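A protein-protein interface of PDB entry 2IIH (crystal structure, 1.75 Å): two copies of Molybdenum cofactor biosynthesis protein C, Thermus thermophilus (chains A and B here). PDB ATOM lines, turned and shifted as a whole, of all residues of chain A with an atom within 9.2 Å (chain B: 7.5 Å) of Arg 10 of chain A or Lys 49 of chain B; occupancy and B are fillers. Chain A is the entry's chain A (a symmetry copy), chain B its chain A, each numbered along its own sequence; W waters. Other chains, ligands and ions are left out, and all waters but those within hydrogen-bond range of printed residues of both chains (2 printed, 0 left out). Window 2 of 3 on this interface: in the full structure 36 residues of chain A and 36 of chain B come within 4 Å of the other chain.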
ATOM      1  N   ARG A  10     -29.321  18.954  -5.136  1.00  0.00           N
ATOM      2  CA  ARG A  10     -28.226  19.434  -6.022  1.00  0.00           C
ATOM      3  C   ARG A  10     -27.301  18.292  -6.438  1.00  0.00           C
ATOM      4  O   ARG A  10     -27.171  17.291  -5.729  1.00  0.00           O
ATOM      5  CB  ARG A  10     -27.417  20.522  -5.307  1.00  0.00           C
ATOM      6  CG  ARG A  10     -26.829  20.086  -3.973  1.00  0.00           C
ATOM      7  CD  ARG A  10     -25.965  21.179  -3.347  1.00  0.00           C
ATOM      8  NE  ARG A  10     -25.312  20.719  -2.123  1.00  0.00           N
ATOM      9  CZ  ARG A  10     -25.923  20.574  -0.951  1.00  0.00           C
ATOM     10  NH1 ARG A  10     -27.210  20.865  -0.826  1.00  0.00           N
ATOM     11  NH2 ARG A  10     -25.248  20.114   0.094  1.00  0.00           N
ATOM     12  N   PRO A  11     -26.656  18.420  -7.607  1.00  0.00           N
ATOM     13  CA  PRO A  11     -25.739  17.392  -8.109  1.00  0.00           C
ATOM     14  C   PRO A  11     -24.555  17.212  -7.164  1.00  0.00           C
ATOM     15  O   PRO A  11     -24.159  18.149  -6.473  1.00  0.00           O
ATOM     16  CB  PRO A  11     -25.294  17.950  -9.457  1.00  0.00           C
ATOM     17  CG  PRO A  11     -26.478  18.770  -9.893  1.00  0.00           C
ATOM     18  CD  PRO A  11     -26.871  19.471  -8.618  1.00  0.00           C
ATOM     19  N   ARG A  12     -23.986  16.013  -7.142  1.00  0.00           N
ATOM     20  CA  ARG A  12     -22.841  15.741  -6.283  1.00  0.00           C
ATOM     21  C   ARG A  12     -22.136  14.448  -6.667  1.00  0.00           C
ATOM     22  O   ARG A  12     -22.763  13.510  -7.159  1.00  0.00           O
ATOM     23  CB  ARG A  12     -23.286  15.641  -4.822  1.00  0.00           C
ATOM     24  CG  ARG A  12     -24.308  14.540  -4.569  1.00  0.00           C
ATOM     25  CD  ARG A  12     -24.391  14.173  -3.093  1.00  0.00           C
ATOM     26  NE  ARG A  12     -24.799  15.292  -2.246  1.00  0.00           N
ATOM     27  CZ  ARG A  12     -25.976  15.904  -2.325  1.00  0.00           C
ATOM     28  NH1 ARG A  12     -26.874  15.513  -3.218  1.00  0.00           N
ATOM     29  NH2 ARG A  12     -26.261  16.904  -1.501  1.00  0.00           N
ATOM     30  N   MET A  13     -20.825  14.407  -6.457  1.00  0.00           N
ATOM     31  CA  MET A  13     -20.070  13.194  -6.740  1.00  0.00           C
ATOM     32  C   MET A  13     -20.181  12.396  -5.447  1.00  0.00           C
ATOM     33  O   MET A  13     -19.466  12.666  -4.476  1.00  0.00           O
ATOM     34  CB  MET A  13     -18.598  13.503  -7.033  1.00  0.00           C
ATOM     35  CG  MET A  13     -17.801  12.279  -7.459  1.00  0.00           C
ATOM     36  SD  MET A  13     -16.012  12.504  -7.434  1.00  0.00           S
ATOM     37  CE  MET A  13     -15.783  13.471  -8.905  1.00  0.00           C
ATOM     38  N   VAL A  14     -21.104  11.438  -5.437  1.00  0.00           N
ATOM     39  CA  VAL A  14     -21.354  10.592  -4.274  1.00  0.00           C
ATOM     40  C   VAL A  14     -20.078  10.215  -3.537  1.00  0.00           C
ATOM     41  O   VAL A  14     -19.090   9.806  -4.148  1.00  0.00           O
ATOM     42  CB  VAL A  14     -22.084   9.293  -4.678  1.00  0.00           C
ATOM     43  CG1 VAL A  14     -22.453   8.496  -3.437  1.00  0.00           C
ATOM     44  CG2 VAL A  14     -23.325   9.624  -5.491  1.00  0.00           C
ATOM     45  N   ASP A  15     -20.106  10.351  -2.216  1.00  0.00           N
ATOM     46  CA  ASP A  15     -18.950  10.025  -1.395  1.00  0.00           C
ATOM     47  C   ASP A  15     -18.834   8.516  -1.212  1.00  0.00           C
ATOM     48  O   ASP A  15     -19.764   7.863  -0.733  1.00  0.00           O
ATOM     49  CB  ASP A  15     -19.058  10.724  -0.034  1.00  0.00           C
ATOM     50  CG  ASP A  15     -17.875  10.430   0.867  1.00  0.00           C
ATOM     51  OD1 ASP A  15     -16.785  10.124   0.342  1.00  0.00           O
ATOM     52  OD2 ASP A  15     -18.029  10.524   2.102  1.00  0.00           O
ATOM     53  N   ILE A  71     -18.219  13.013 -18.181  1.00  0.00           N
ATOM     54  CA  ILE A  71     -19.406  12.775 -17.369  1.00  0.00           C
ATOM     55  C   ILE A  71     -19.219  13.527 -16.045  1.00  0.00           C
ATOM     56  O   ILE A  71     -18.436  13.113 -15.181  1.00  0.00           O
ATOM     57  CB  ILE A  71     -19.576  11.266 -17.145  1.00  0.00           C
ATOM     58  CG1 ILE A  71     -19.511  10.547 -18.500  1.00  0.00           C
ATOM     59  CG2 ILE A  71     -20.898  10.977 -16.469  1.00  0.00           C
ATOM     60  CD1 ILE A  71     -19.549   9.053 -18.383  1.00  0.00           C
ATOM     61  N   PRO A  72     -19.952  14.641 -15.873  1.00  0.00           N
ATOM     62  CA  PRO A  72     -19.899  15.508 -14.692  1.00  0.00           C
ATOM     63  C   PRO A  72     -19.720  14.904 -13.305  1.00  0.00           C
ATOM     64  O   PRO A  72     -18.777  15.254 -12.605  1.00  0.00           O
ATOM     65  CB  PRO A  72     -21.186  16.327 -14.809  1.00  0.00           C
ATOM     66  CG  PRO A  72     -21.322  16.492 -16.289  1.00  0.00           C
ATOM     67  CD  PRO A  72     -21.035  15.075 -16.778  1.00  0.00           C
ATOM     68  N   LEU A  73     -20.602  13.993 -12.902  1.00  0.00           N
ATOM     69  CA  LEU A  73     -20.510  13.415 -11.566  1.00  0.00           C
ATOM     70  C   LEU A  73     -19.708  12.122 -11.441  1.00  0.00           C
ATOM     71  O   LEU A  73     -19.654  11.511 -10.368  1.00  0.00           O
ATOM     72  CB  LEU A  73     -21.921  13.206 -11.007  1.00  0.00           C
ATOM     73  CG  LEU A  73     -22.813  14.447 -11.067  1.00  0.00           C
ATOM     74  CD1 LEU A  73     -24.203  14.106 -10.528  1.00  0.00           C
ATOM     75  CD2 LEU A  73     -22.177  15.587 -10.272  1.00  0.00           C
ATOM     76  N   CYS A  74     -19.059  11.726 -12.526  1.00  0.00           N
ATOM     77  CA  CYS A  74     -18.266  10.502 -12.567  1.00  0.00           C
ATOM     78  C   CYS A  74     -16.989  10.584 -11.727  1.00  0.00           C
ATOM     79  O   CYS A  74     -16.302  11.608 -11.722  1.00  0.00           O
ATOM     80  CB  CYS A  74     -17.917  10.184 -14.022  1.00  0.00           C
ATOM     81  SG  CYS A  74     -16.992   8.664 -14.284  1.00  0.00           S
ATOM     82  N   HIS A  75     -16.673   9.501 -11.022  1.00  0.00           N
ATOM     83  CA  HIS A  75     -15.477   9.446 -10.175  1.00  0.00           C
ATOM     84  C   HIS A  75     -14.211   9.184 -10.992  1.00  0.00           C
ATOM     85  O   HIS A  75     -14.169   8.264 -11.808  1.00  0.00           O
ATOM     86  CB  HIS A  75     -15.596   8.330  -9.121  1.00  0.00           C
ATOM     87  CG  HIS A  75     -16.756   8.485  -8.183  1.00  0.00           C
ATOM     88  ND1 HIS A  75     -18.053   8.211  -8.550  1.00  0.00           N
ATOM     89  CD2 HIS A  75     -16.805   8.882  -6.889  1.00  0.00           C
ATOM     90  CE1 HIS A  75     -18.858   8.431  -7.522  1.00  0.00           C
ATOM     91  NE2 HIS A  75     -18.123   8.839  -6.503  1.00  0.00           N
ATOM     92  N   THR A 107     -16.042   2.446  -6.840  1.00  0.00           N
ATOM     93  CA  THR A 107     -17.171   2.661  -7.738  1.00  0.00           C
ATOM     94  C   THR A 107     -16.958   1.855  -9.018  1.00  0.00           C
ATOM     95  O   THR A 107     -15.840   1.428  -9.310  1.00  0.00           O
ATOM     96  CB  THR A 107     -17.331   4.160  -8.087  1.00  0.00           C
ATOM     97  OG1 THR A 107     -16.070   4.690  -8.506  1.00  0.00           O
ATOM     98  CG2 THR A 107     -17.826   4.942  -6.876  1.00  0.00           C
ATOM     99  N   MET A 111     -19.631   3.525 -16.771  1.00  0.00           N
ATOM    100  CA  MET A 111     -19.518   4.707 -17.617  1.00  0.00           C
ATOM    101  C   MET A 111     -18.330   4.637 -18.560  1.00  0.00           C
ATOM    102  O   MET A 111     -18.416   5.086 -19.698  1.00  0.00           O
ATOM    103  CB  MET A 111     -19.440   5.984 -16.775  1.00  0.00           C
ATOM    104  CG  MET A 111     -20.731   6.333 -16.062  1.00  0.00           C
ATOM    105  SD  MET A 111     -22.211   6.013 -17.072  1.00  0.00           S
ATOM    106  CE  MET A 111     -21.927   7.022 -18.511  1.00  0.00           C
ATOM    107  N   GLY B  45     -36.877  14.226  -9.803  1.00  0.00           N
ATOM    108  CA  GLY B  45     -35.631  14.968  -9.748  1.00  0.00           C
ATOM    109  C   GLY B  45     -34.390  14.102  -9.636  1.00  0.00           C
ATOM    110  O   GLY B  45     -33.281  14.619  -9.493  1.00  0.00           O
ATOM    111  N   GLY B  46     -34.571  12.787  -9.695  1.00  0.00           N
ATOM    112  CA  GLY B  46     -33.438  11.882  -9.600  1.00  0.00           C
ATOM    113  C   GLY B  46     -33.534  10.912  -8.438  1.00  0.00           C
ATOM    114  O   GLY B  46     -34.574  10.813  -7.786  1.00  0.00           O
ATOM    115  N   VAL B  47     -32.445  10.193  -8.184  1.00  0.00           N
ATOM    116  CA  VAL B  47     -32.392   9.219  -7.097  1.00  0.00           C
ATOM    117  C   VAL B  47     -31.226   9.507  -6.151  1.00  0.00           C
ATOM    118  O   VAL B  47     -30.356   8.661  -5.943  1.00  0.00           O
ATOM    119  CB  VAL B  47     -32.249   7.781  -7.647  1.00  0.00           C
ATOM    120  CG1 VAL B  47     -33.510   7.385  -8.393  1.00  0.00           C
ATOM    121  CG2 VAL B  47     -31.045   7.692  -8.577  1.00  0.00           C
ATOM    122  N   GLY B  48     -31.221  10.711  -5.581  1.00  0.00           N
ATOM    123  CA  GLY B  48     -30.165  11.098  -4.662  1.00  0.00           C
ATOM    124  C   GLY B  48     -28.849  11.358  -5.369  1.00  0.00           C
ATOM    125  O   GLY B  48     -27.853  10.679  -5.109  1.00  0.00           O
ATOM    126  N   LYS B  49     -28.838  12.347  -6.261  1.00  0.00           N
ATOM    127  CA  LYS B  49     -27.628  12.670  -7.005  1.00  0.00           C
ATOM    128  C   LYS B  49     -27.770  13.937  -7.846  1.00  0.00           C
ATOM    129  O   LYS B  49     -26.785  14.443  -8.382  1.00  0.00           O
ATOM    130  CB  LYS B  49     -27.261  11.502  -7.923  1.00  0.00           C
ATOM    131  CG  LYS B  49     -25.877  11.596  -8.539  1.00  0.00           C
ATOM    132  CD  LYS B  49     -25.687  10.545  -9.621  1.00  0.00           C
ATOM    133  CE  LYS B  49     -24.211  10.311  -9.899  1.00  0.00           C
ATOM    134  NZ  LYS B  49     -24.010   9.437 -11.082  1.00  0.00           N
ATOM    135  N   GLY B  50     -28.995  14.443  -7.965  1.00  0.00           N
ATOM    136  CA  GLY B  50     -29.227  15.638  -8.757  1.00  0.00           C
ATOM    137  C   GLY B  50     -30.163  15.360  -9.921  1.00  0.00           C
ATOM    138  O   GLY B  50     -30.480  14.203 -10.196  1.00  0.00           O
ATOM    139  N   ASP B  51     -30.602  16.415 -10.604  1.00  0.00           N
ATOM    140  CA  ASP B  51     -31.515  16.279 -11.739  1.00  0.00           C
ATOM    141  C   ASP B  51     -30.760  15.822 -12.986  1.00  0.00           C
ATOM    142  O   ASP B  51     -29.972  16.576 -13.559  1.00  0.00           O
ATOM    143  CB  ASP B  51     -32.196  17.620 -12.029  1.00  0.00           C
ATOM    144  CG  ASP B  51     -33.401  17.482 -12.942  1.00  0.00           C
ATOM    145  OD1 ASP B  51     -33.336  16.695 -13.907  1.00  0.00           O
ATOM    146  OD2 ASP B  51     -34.411  18.175 -12.699  1.00  0.00           O
ATOM    147  N   PRO B  52     -31.003  14.579 -13.431  1.00  0.00           N
ATOM    148  CA  PRO B  52     -30.327  14.042 -14.617  1.00  0.00           C
ATOM    149  C   PRO B  52     -30.447  14.903 -15.877  1.00  0.00           C
ATOM    150  O   PRO B  52     -29.482  15.052 -16.624  1.00  0.00           O
ATOM    151  CB  PRO B  52     -30.982  12.672 -14.792  1.00  0.00           C
ATOM    152  CG  PRO B  52     -31.339  12.285 -13.384  1.00  0.00           C
ATOM    153  CD  PRO B  52     -31.910  13.576 -12.848  1.00  0.00           C
ATOM    154  N   VAL B  55     -28.075  18.178 -15.501  1.00  0.00           N
ATOM    155  CA  VAL B  55     -26.655  17.851 -15.577  1.00  0.00           C
ATOM    156  C   VAL B  55     -26.278  17.389 -16.983  1.00  0.00           C
ATOM    157  O   VAL B  55     -25.216  17.739 -17.497  1.00  0.00           O
ATOM    158  CB  VAL B  55     -26.297  16.755 -14.543  1.00  0.00           C
ATOM    159  CG1 VAL B  55     -24.822  16.380 -14.649  1.00  0.00           C
ATOM    160  CG2 VAL B  55     -26.609  17.263 -13.134  1.00  0.00           C
ATOM    161  N   THR B 123     -24.724  10.922 -19.926  1.00  0.00           N
ATOM    162  CA  THR B 123     -24.878  11.531 -18.611  1.00  0.00           C
ATOM    163  C   THR B 123     -26.233  11.189 -18.012  1.00  0.00           C
ATOM    164  O   THR B 123     -26.350  10.969 -16.807  1.00  0.00           O
ATOM    165  CB  THR B 123     -24.679  13.044 -18.698  1.00  0.00           C
ATOM    166  OG1 THR B 123     -23.355  13.297 -19.181  1.00  0.00           O
ATOM    167  CG2 THR B 123     -24.845  13.693 -17.331  1.00  0.00           C
ATOM    168  N   TYR B 125     -27.765   8.469 -18.590  1.00  0.00           N
ATOM    169  CA  TYR B 125     -27.558   7.084 -18.178  1.00  0.00           C
ATOM    170  C   TYR B 125     -26.802   7.031 -16.852  1.00  0.00           C
ATOM    171  O   TYR B 125     -27.178   6.298 -15.935  1.00  0.00           O
ATOM    172  CB  TYR B 125     -26.750   6.318 -19.237  1.00  0.00           C
ATOM    173  CG  TYR B 125     -26.420   4.898 -18.830  1.00  0.00           C
ATOM    174  CD1 TYR B 125     -27.375   3.886 -18.920  1.00  0.00           C
ATOM    175  CD2 TYR B 125     -25.170   4.577 -18.296  1.00  0.00           C
ATOM    176  CE1 TYR B 125     -27.092   2.587 -18.485  1.00  0.00           C
ATOM    177  CE2 TYR B 125     -24.879   3.283 -17.859  1.00  0.00           C
ATOM    178  CZ  TYR B 125     -25.847   2.295 -17.954  1.00  0.00           C
ATOM    179  OH  TYR B 125     -25.576   1.023 -17.500  1.00  0.00           O
ATOM    180  N   ASP B 126     -25.731   7.816 -16.748  1.00  0.00           N
ATOM    181  CA  ASP B 126     -24.928   7.822 -15.530  1.00  0.00           C
ATOM    182  C   ASP B 126     -25.743   8.089 -14.277  1.00  0.00           C
ATOM    183  O   ASP B 126     -25.545   7.452 -13.246  1.00  0.00           O
ATOM    184  CB  ASP B 126     -23.815   8.872 -15.612  1.00  0.00           C
ATOM    185  CG  ASP B 126     -23.022   8.979 -14.314  1.00  0.00           C
ATOM    186  OD1 ASP B 126     -22.484   7.946 -13.869  1.00  0.00           O
ATOM    187  OD2 ASP B 126     -22.945  10.087 -13.736  1.00  0.00           O
ATOM    188  N   MET B 127     -26.675   9.023 -14.370  1.00  0.00           N
ATOM    189  CA  MET B 127     -27.462   9.370 -13.200  1.00  0.00           C
ATOM    190  C   MET B 127     -28.743   8.587 -12.960  1.00  0.00           C
ATOM    191  O   MET B 127     -29.469   8.864 -12.010  1.00  0.00           O
ATOM    192  CB  MET B 127     -27.723  10.864 -13.224  1.00  0.00           C
ATOM    193  CG  MET B 127     -26.429  11.628 -13.008  1.00  0.00           C
ATOM    194  SD  MET B 127     -26.583  13.342 -13.366  1.00  0.00           S
ATOM    195  CE  MET B 127     -27.576  13.873 -11.979  1.00  0.00           C
ATOM    196  N   LEU B 128     -29.005   7.597 -13.805  1.00  0.00           N
ATOM    197  CA  LEU B 128     -30.191   6.758 -13.648  1.00  0.00           C
ATOM    198  C   LEU B 128     -29.813   5.283 -13.598  1.00  0.00           C
ATOM    199  O   LEU B 128     -30.654   4.433 -13.308  1.00  0.00           O
ATOM    200  CB  LEU B 128     -31.174   6.980 -14.799  1.00  0.00           C
ATOM    201  CG  LEU B 128     -31.909   8.317 -14.881  1.00  0.00           C
ATOM    202  CD1 LEU B 128     -32.757   8.342 -16.142  1.00  0.00           C
ATOM    203  CD2 LEU B 128     -32.775   8.511 -13.646  1.00  0.00           C
ATOM    204  N   LYS B 129     -28.547   4.976 -13.865  1.00  0.00           N
ATOM    205  CA  LYS B 129     -28.098   3.586 -13.863  1.00  0.00           C
ATOM    206  C   LYS B 129     -28.152   2.923 -12.488  1.00  0.00           C
ATOM    207  O   LYS B 129     -28.117   1.697 -12.383  1.00  0.00           O
ATOM    208  CB  LYS B 129     -26.679   3.479 -14.436  1.00  0.00           C
ATOM    209  CG  LYS B 129     -25.571   3.980 -13.527  1.00  0.00           C
ATOM    210  CD  LYS B 129     -24.221   3.826 -14.214  1.00  0.00           C
ATOM    211  CE  LYS B 129     -23.068   4.084 -13.262  1.00  0.00           C
ATOM    212  NZ  LYS B 129     -23.174   5.412 -12.611  1.00  0.00           N
ATOM    213  N   ALA B 130     -28.236   3.731 -11.436  1.00  0.00           N
ATOM    214  CA  ALA B 130     -28.302   3.193 -10.083  1.00  0.00           C
ATOM    215  C   ALA B 130     -29.605   2.418  -9.910  1.00  0.00           C
ATOM    216  O   ALA B 130     -29.653   1.414  -9.200  1.00  0.00           O
ATOM    217  CB  ALA B 130     -28.225   4.321  -9.063  1.00  0.00           C
HETATM  218  O   HOH W   1     -23.068  12.856 -14.205  1.00  0.00           O
HETATM  219  O   HOH W   2     -29.024  14.125  -4.131  1.00  0.00           O
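Of the printed residues of chain B, Arg 10 of chain A touches Lys 49.
Of chain A, only Arg 10, Pro 11, Arg 12 and Leu 73 come within 4 Å of Lys 49 of chain B.
Of the printed residues of chain B, Leu 73 of chain A touches Lys 49 (3.4 Å) and Met 127 (3.7 Å).
Of the printed residues of chain A, Thr 123 of chain B touches Pro 72.
Printed residues of chain A within 4 Å of Val 55 of chain B: Pro 11 and Pro 72.
Printed residues of chain B within 4 Å of Met 111 of chain A: Tyr 125 and Asp 126.
Printed residues of chain B within 4 Å of Arg 12 of chain A: Lys 49.
Asp 51 of chain B touches none of the printed residues of chain A.
Gly 45 of chain B touches none of the printed residues of chain A.
The nearest printed residue of chain B that does not touch Arg 10 of chain A is Gly 50 of chain B (4.02 Å).
The nearest residue of chain A that does not touch Lys 49 of chain B is Val 14 of chain A (4.4 Å).
The nearest printed residue of chain A that does not touch Val 55 of chain B is Leu 73 of chain A (4.5 Å).
O of Lys 49 of chain B touches O of Arg 10 of chain A, at 3.9 Å.
Lys 49 of chain B touches Pro 11 of chain A.
Gly 50 of chain B touches Pro 11 of chain A (CA to CA, 3.96 Å).
CG of Pro 11 of chain A touches CG2 of Val 55 of chain B, 3.6 Å away.
Ile 71 of chain A touches Asp 126 of chain B (CG2 to OD2, 3.5 Å).
Pro 72 of chain A touches Val 55 of chain B (CB to CG1, 3.6 Å).
Pro 72 of chain A touches Thr 123 of chain B (CD to OG1, 3.8 Å).
Lys 49 of chain B touches Leu 73 of chain A (O to CD1, 3.4 Å).
Met 127 of chain B touches Leu 73 of chain A (CE to CD1, 3.7 Å).
CD2 of Tyr 125 of chain B touches SD of Met 111 of chain A, 3.5 Å away.
Water W2 bridges the guanidinium group of Arg 12 of chain A (2.7 Å) and the backbone NH of Lys 49 of chain B (2.8 Å).
Water W1 lies within hydrogen-bond range of OD2 of Asp 126 of chain B (2.8 Å), N of Leu 73 of chain A (3.0 Å) and SD of Met 127 of chain B (3.6 Å).
NZ of Lys 49 of chain B is in salt-bridge range of OD2 of Asp 126 of chain B (2.9 Å).
The side-chain carboxylate (OD1) of Asp 126 of chain B is in salt-bridge range of the side-chain amino group (NZ) of Lys 129 of chain B.
The backbone carbonyl oxygen (O) of Arg 10 of chain A sits at hydrogen-bond distance from the guanidinium group (NH1) of Arg 12 of chain A (3.1 Å).
No position is printed for both chains.
O of Lys 49 of chain B is in hydrogen-bond range of N of Arg 12 of chain A, 3.4 Å away.
The side-chain carboxylate (OD1) of Asp 126 of chain B sits close to the side-chain sulfur (SD) of Met 111 of chain A.
Of the 13 printed residues of chain A, 7 touch a printed residue of chain B.
Hydrophobic or aromatic side chains of chain A that line the printed part of chain B: Pro 11, Ile 71, Pro 72, Leu 73 and Met 111.
Hydrophobic or aromatic side chains of chain B that line the printed part of chain A: Val 55, Tyr 125 and Met 127.
Along chain B the printed residues that touch a printed residue of chain A span positions 49 to 127.
Among the printed residues, no Asp or Glu carboxylate lies within 4 Å of a Lys or Arg side-chain nitrogen of the other chain.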
